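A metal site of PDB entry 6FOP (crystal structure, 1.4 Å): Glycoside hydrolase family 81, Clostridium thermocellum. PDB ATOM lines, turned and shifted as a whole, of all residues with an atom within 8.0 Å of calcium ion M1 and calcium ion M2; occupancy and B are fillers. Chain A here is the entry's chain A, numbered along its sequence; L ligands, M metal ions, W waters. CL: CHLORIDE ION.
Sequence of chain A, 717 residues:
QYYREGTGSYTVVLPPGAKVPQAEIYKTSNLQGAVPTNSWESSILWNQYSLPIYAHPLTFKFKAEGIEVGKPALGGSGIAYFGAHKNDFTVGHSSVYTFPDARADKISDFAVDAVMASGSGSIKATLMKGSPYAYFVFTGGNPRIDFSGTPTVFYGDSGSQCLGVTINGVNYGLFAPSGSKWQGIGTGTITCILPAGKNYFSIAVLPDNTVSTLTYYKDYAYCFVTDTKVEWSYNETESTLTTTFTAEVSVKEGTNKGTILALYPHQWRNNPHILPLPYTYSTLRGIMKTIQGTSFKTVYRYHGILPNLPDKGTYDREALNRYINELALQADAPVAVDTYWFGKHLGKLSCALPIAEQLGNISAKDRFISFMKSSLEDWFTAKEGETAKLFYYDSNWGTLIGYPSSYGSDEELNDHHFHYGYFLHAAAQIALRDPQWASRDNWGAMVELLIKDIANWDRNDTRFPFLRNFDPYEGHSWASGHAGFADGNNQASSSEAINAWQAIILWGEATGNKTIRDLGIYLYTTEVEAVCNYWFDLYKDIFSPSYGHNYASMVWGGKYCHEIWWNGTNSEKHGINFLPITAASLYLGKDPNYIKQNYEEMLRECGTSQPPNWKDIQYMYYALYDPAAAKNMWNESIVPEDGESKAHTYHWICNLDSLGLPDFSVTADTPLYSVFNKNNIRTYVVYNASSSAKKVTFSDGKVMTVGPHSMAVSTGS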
ATOM      1  N   SER A   9      11.699   3.203   3.749  1.00  0.00           N
ATOM      2  CA  SER A   9      11.941   3.071   2.333  1.00  0.00           C
ATOM      3  C   SER A   9      13.068   2.109   2.069  1.00  0.00           C
ATOM      4  O   SER A   9      13.908   1.882   2.953  1.00  0.00           O
ATOM      5  CB  SER A   9      12.294   4.435   1.721  1.00  0.00           C
ATOM      6  OG  SER A   9      13.493   4.953   2.296  1.00  0.00           O
ATOM      7  N   SER A 374      16.179   4.056  16.938  1.00  0.00           N
ATOM      8  CA  SER A 374      16.855   4.968  16.014  1.00  0.00           C
ATOM      9  C   SER A 374      17.632   4.163  14.955  1.00  0.00           C
ATOM     10  O   SER A 374      17.653   4.546  13.771  1.00  0.00           O
ATOM     11  CB  SER A 374      17.763   5.944  16.752  1.00  0.00           C
ATOM     12  OG  SER A 374      18.818   5.293  17.439  1.00  0.00           O
ATOM     13  N   SER A 375      18.244   3.061  15.363  1.00  0.00           N
ATOM     14  CA  SER A 375      19.016   2.307  14.391  1.00  0.00           C
ATOM     15  C   SER A 375      18.105   1.567  13.406  1.00  0.00           C
ATOM     16  O   SER A 375      18.423   1.571  12.224  1.00  0.00           O
ATOM     17  CB  SER A 375      20.022   1.386  15.045  1.00  0.00           C
ATOM     18  OG  SER A 375      19.367   0.347  15.728  1.00  0.00           O
ATOM     19  N   LEU A 376      17.002   0.981  13.871  1.00  0.00           N
ATOM     20  CA  LEU A 376      16.052   0.346  12.960  1.00  0.00           C
ATOM     21  C   LEU A 376      15.455   1.373  11.997  1.00  0.00           C
ATOM     22  O   LEU A 376      15.319   1.105  10.801  1.00  0.00           O
ATOM     23  CB  LEU A 376      14.973  -0.435  13.690  1.00  0.00           C
ATOM     24  CG  LEU A 376      15.448  -1.726  14.327  1.00  0.00           C
ATOM     25  CD1 LEU A 376      14.321  -2.327  15.116  1.00  0.00           C
ATOM     26  CD2 LEU A 376      16.017  -2.724  13.306  1.00  0.00           C
ATOM     27  N   GLU A 377      15.117   2.551  12.504  1.00  0.00           N
ATOM     28  CA  GLU A 377      14.534   3.588  11.643  1.00  0.00           C
ATOM     29  C   GLU A 377      15.557   3.994  10.564  1.00  0.00           C
ATOM     30  O   GLU A 377      15.198   4.192   9.414  1.00  0.00           O
ATOM     31  CB  GLU A 377      14.062   4.778  12.471  1.00  0.00           C
ATOM     32  CG  GLU A 377      12.916   4.445  13.417  1.00  0.00           C
ATOM     33  CD  GLU A 377      12.588   5.528  14.425  1.00  0.00           C
ATOM     34  OE1 GLU A 377      12.988   6.691  14.216  1.00  0.00           O
ATOM     35  OE2 GLU A 377      11.892   5.205  15.407  1.00  0.00           O
ATOM     36  N   ASP A 378      16.831   4.052  10.920  1.00  0.00           N
ATOM     37  CA  ASP A 378      17.914   4.357   9.958  1.00  0.00           C
ATOM     38  C   ASP A 378      18.011   3.208   8.913  1.00  0.00           C
ATOM     39  O   ASP A 378      17.901   3.436   7.704  1.00  0.00           O
ATOM     40  CB  ASP A 378      19.248   4.622  10.692  1.00  0.00           C
ATOM     41  CG  ASP A 378      20.360   5.114   9.771  1.00  0.00           C
ATOM     42  OD1 ASP A 378      20.260   5.030   8.508  1.00  0.00           O
ATOM     43  OD2 ASP A 378      21.358   5.632  10.313  1.00  0.00           O
ATOM     44  N   TRP A 379      18.169   1.990   9.394  1.00  0.00           N
ATOM     45  CA  TRP A 379      18.265   0.862   8.468  1.00  0.00           C
ATOM     46  C   TRP A 379      17.072   0.786   7.554  1.00  0.00           C
ATOM     47  O   TRP A 379      17.221   0.392   6.391  1.00  0.00           O
ATOM     48  CB  TRP A 379      18.481  -0.460   9.214  1.00  0.00           C
ATOM     49  CG  TRP A 379      19.909  -0.731   9.623  1.00  0.00           C
ATOM     50  CD1 TRP A 379      20.501  -0.464  10.827  1.00  0.00           C
ATOM     51  CD2 TRP A 379      20.928  -1.328   8.819  1.00  0.00           C
ATOM     52  NE1 TRP A 379      21.802  -0.860  10.814  1.00  0.00           N
ATOM     53  CE2 TRP A 379      22.089  -1.415   9.591  1.00  0.00           C
ATOM     54  CE3 TRP A 379      20.954  -1.829   7.513  1.00  0.00           C
ATOM     55  CZ2 TRP A 379      23.273  -1.945   9.090  1.00  0.00           C
ATOM     56  CZ3 TRP A 379      22.117  -2.344   7.027  1.00  0.00           C
ATOM     57  CH2 TRP A 379      23.256  -2.421   7.804  1.00  0.00           C
ATOM     58  N   PHE A 380      15.873   1.094   8.073  1.00  0.00           N
ATOM     59  CA  PHE A 380      14.618   0.981   7.331  1.00  0.00           C
ATOM     60  C   PHE A 380      14.290   2.197   6.478  1.00  0.00           C
ATOM     61  O   PHE A 380      13.176   2.289   5.956  1.00  0.00           O
ATOM     62  CB  PHE A 380      13.436   0.651   8.275  1.00  0.00           C
ATOM     63  CG  PHE A 380      13.514  -0.688   8.961  1.00  0.00           C
ATOM     64  CD1 PHE A 380      14.275  -1.743   8.462  1.00  0.00           C
ATOM     65  CD2 PHE A 380      12.764  -0.903  10.112  1.00  0.00           C
ATOM     66  CE1 PHE A 380      14.304  -2.975   9.100  1.00  0.00           C
ATOM     67  CE2 PHE A 380      12.783  -2.119  10.739  1.00  0.00           C
ATOM     68  CZ  PHE A 380      13.557  -3.160  10.230  1.00  0.00           C
ATOM     69  N   THR A 381      15.271   3.104   6.304  1.00  0.00           N
ATOM     70  CA  THR A 381      15.154   4.246   5.414  1.00  0.00           C
ATOM     71  C   THR A 381      16.392   4.296   4.503  1.00  0.00           C
ATOM     72  O   THR A 381      17.518   4.270   4.979  1.00  0.00           O
ATOM     73  CB  THR A 381      15.091   5.553   6.241  1.00  0.00           C
ATOM     74  OG1 THR A 381      14.024   5.459   7.192  1.00  0.00           O
ATOM     75  CG2 THR A 381      14.869   6.744   5.343  1.00  0.00           C
ATOM     76  N   ALA A 382      16.177   4.343   3.201  1.00  0.00           N
ATOM     77  CA  ALA A 382      17.248   4.461   2.222  1.00  0.00           C
ATOM     78  C   ALA A 382      17.267   5.886   1.705  1.00  0.00           C
ATOM     79  O   ALA A 382      16.438   6.276   0.867  1.00  0.00           O
ATOM     80  CB  ALA A 382      17.037   3.467   1.063  1.00  0.00           C
ATOM     81  N   LYS A 383      18.181   6.687   2.224  1.00  0.00           N
ATOM     82  CA  LYS A 383      18.318   8.087   1.809  1.00  0.00           C
ATOM     83  C   LYS A 383      19.152   8.213   0.536  1.00  0.00           C
ATOM     84  O   LYS A 383      20.023   7.407   0.276  1.00  0.00           O
ATOM     85  CB  LYS A 383      18.938   8.926   2.935  1.00  0.00           C
ATOM     86  CG  LYS A 383      17.986   9.145   4.094  1.00  0.00           C
ATOM     87  CD  LYS A 383      18.580  10.117   5.106  1.00  0.00           C
ATOM     88  CE  LYS A 383      17.535  10.493   6.159  1.00  0.00           C
ATOM     89  NZ  LYS A 383      18.094  11.439   7.152  1.00  0.00           N
ATOM     90  N   GLU A 386      23.049   7.698   0.450  1.00  0.00           N
ATOM     91  CA  GLU A 386      23.458   6.998   1.664  1.00  0.00           C
ATOM     92  C   GLU A 386      24.153   5.717   1.236  1.00  0.00           C
ATOM     93  O   GLU A 386      23.702   5.051   0.303  1.00  0.00           O
ATOM     94  CB  GLU A 386      22.233   6.683   2.526  1.00  0.00           C
ATOM     95  CG  GLU A 386      22.556   6.210   3.925  1.00  0.00           C
ATOM     96  CD  GLU A 386      21.328   5.919   4.771  1.00  0.00           C
ATOM     97  OE1 GLU A 386      20.259   5.551   4.212  1.00  0.00           O
ATOM     98  OE2 GLU A 386      21.415   5.972   6.017  1.00  0.00           O
ATOM     99  N   THR A 387      25.257   5.367   1.886  1.00  0.00           N
ATOM    100  CA  THR A 387      25.999   4.163   1.525  1.00  0.00           C
ATOM    101  C   THR A 387      26.018   3.078   2.583  1.00  0.00           C
ATOM    102  O   THR A 387      26.468   1.952   2.306  1.00  0.00           O
ATOM    103  CB  THR A 387      27.446   4.511   1.195  1.00  0.00           C
ATOM    104  OG1 THR A 387      28.036   5.191   2.297  1.00  0.00           O
ATOM    105  CG2 THR A 387      27.503   5.397  -0.043  1.00  0.00           C
ATOM    106  N   ALA A 388      25.551   3.403   3.784  1.00  0.00           N
ATOM    107  CA  ALA A 388      25.468   2.431   4.864  1.00  0.00           C
ATOM    108  C   ALA A 388      24.148   2.603   5.600  1.00  0.00           C
ATOM    109  O   ALA A 388      23.614   3.702   5.678  1.00  0.00           O
ATOM    110  CB  ALA A 388      26.619   2.612   5.828  1.00  0.00           C
ATOM    111  N   LYS A 389      23.658   1.489   6.114  1.00  0.00           N
ATOM    112  CA  LYS A 389      22.449   1.409   6.888  1.00  0.00           C
ATOM    113  C   LYS A 389      21.246   1.698   5.991  1.00  0.00           C
ATOM    114  O   LYS A 389      20.518   2.657   6.155  1.00  0.00           O
ATOM    115  CB  LYS A 389      22.453   2.267   8.167  1.00  0.00           C
ATOM    116  CG  LYS A 389      23.626   1.999   9.075  1.00  0.00           C
ATOM    117  CD  LYS A 389      23.531   2.842  10.353  1.00  0.00           C
ATOM    118  CE  LYS A 389      24.600   2.454  11.345  1.00  0.00           C
ATOM    119  NZ  LYS A 389      25.993   2.614  10.829  1.00  0.00           N
ATOM    120  N   LEU A 390      21.066   0.778   5.047  1.00  0.00           N
ATOM    121  CA  LEU A 390      19.972   0.839   4.086  1.00  0.00           C
ATOM    122  C   LEU A 390      19.759  -0.531   3.500  1.00  0.00           C
ATOM    123  O   LEU A 390      20.660  -1.404   3.565  1.00  0.00           O
ATOM    124  CB  LEU A 390      20.252   1.864   2.955  1.00  0.00           C
ATOM    125  CG  LEU A 390      21.498   1.496   2.125  1.00  0.00           C
ATOM    126  CD1 LEU A 390      21.143   0.800   0.812  1.00  0.00           C
ATOM    127  CD2 LEU A 390      22.465   2.617   1.927  1.00  0.00           C
ATOM    128  N   PHE A 391      18.568  -0.730   2.948  1.00  0.00           N
ATOM    129  CA  PHE A 391      18.215  -1.935   2.202  1.00  0.00           C
ATOM    130  C   PHE A 391      18.007  -1.624   0.731  1.00  0.00           C
ATOM    131  O   PHE A 391      17.346  -0.655   0.379  1.00  0.00           O
ATOM    132  CB  PHE A 391      16.960  -2.630   2.792  1.00  0.00           C
ATOM    133  CG  PHE A 391      17.242  -3.337   4.109  1.00  0.00           C
ATOM    134  CD1 PHE A 391      17.832  -4.601   4.119  1.00  0.00           C
ATOM    135  CD2 PHE A 391      17.006  -2.714   5.322  1.00  0.00           C
ATOM    136  CE1 PHE A 391      18.147  -5.228   5.308  1.00  0.00           C
ATOM    137  CE2 PHE A 391      17.314  -3.352   6.507  1.00  0.00           C
ATOM    138  CZ  PHE A 391      17.915  -4.592   6.500  1.00  0.00           C
ATOM    139  N   TYR A 403      23.082  -3.099   3.289  1.00  0.00           N
ATOM    140  CA  TYR A 403      24.474  -2.621   3.137  1.00  0.00           C
ATOM    141  C   TYR A 403      24.852  -1.781   4.351  1.00  0.00           C
ATOM    142  O   TYR A 403      24.063  -0.924   4.732  1.00  0.00           O
ATOM    143  CB  TYR A 403      24.686  -1.842   1.849  1.00  0.00           C
ATOM    144  CG  TYR A 403      24.544  -2.706   0.613  1.00  0.00           C
ATOM    145  CD1 TYR A 403      25.455  -3.734   0.335  1.00  0.00           C
ATOM    146  CD2 TYR A 403      23.477  -2.546  -0.235  1.00  0.00           C
ATOM    147  CE1 TYR A 403      25.283  -4.558  -0.771  1.00  0.00           C
ATOM    148  CE2 TYR A 403      23.318  -3.357  -1.350  1.00  0.00           C
ATOM    149  CZ  TYR A 403      24.220  -4.351  -1.614  1.00  0.00           C
ATOM    150  OH  TYR A 403      24.005  -5.120  -2.746  1.00  0.00           O
HETATM  151 CL    CL L   1      18.403   6.846   6.864  1.00  0.00          CL
HETATM  152 CA    CA M   1      19.376   4.697   6.360  1.00  0.00          CA
HETATM  153 CA    CA M   2      22.081   6.797   8.123  1.00  0.00          CA
HETATM  154  O   HOH W   1      23.856   5.618   7.599  1.00  0.00           O
HETATM  155  O   HOH W   2      20.271   8.290   8.445  1.00  0.00           O
HETATM  156  O   HOH W   3      22.777   8.737   6.870  1.00  0.00           O
HETATM  157  O   HOH W   4      23.374   7.943   9.661  1.00  0.00           O
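The side-chain hydroxyl of Thr 381 sits at hydrogen-bond distance from the backbone carbonyl oxygen of Glu 377, 2.8 Å away. The side-chain carboxylate (OE1) of Glu 386 sits close to the backbone NH (N) of Lys 383, 3.1 Å away. N of Lys 389 sits at hydrogen-bond distance from O of Tyr 403, 2.8 Å away.
Four residues have an atom within 4 Å of calcium ion M1: Asp 378, Thr 381, Glu 386 and Lys 389. The nearest printed residue that does not touch calcium ion M1 is Trp 379 (4.2 Å).
OD1 of Asp 378 is bound to calcium ion M1, 2.3 Å away. O of Lys 389 binds calcium ion M1. Calcium ion M1 is bound by O of Thr 381 (2.4 Å). The backbone carbonyl oxygen (O) of Asp 378 is bound to calcium ion M1 (2.4 Å). CL of the ligand is bound to calcium ion M1, 2.4 Å away. Calcium ion M1 is bound by OE2 of Glu 386, 2.4 Å away. OE1 of Glu 386 binds calcium ion M1. Calcium ion M1 has seven donor atoms within binding distance.
Calcium ion M2 is bound by water W1 (2.2 Å), water W4 (2.3 Å), OE2 of Glu 386 (2.4 Å), water W2 (2.4 Å), water W3 (2.4 Å), OD1 of Asp 378 (2.6 Å) and OD2 of Asp 378 (2.6 Å). Calcium ion M2 has seven donor atoms within binding distance.
Two residues have an atom within 4 Å of calcium ion M2: Asp 378 and Glu 386. The nearest printed residue that does not touch calcium ion M2 is Ala 388 (4.2 Å).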
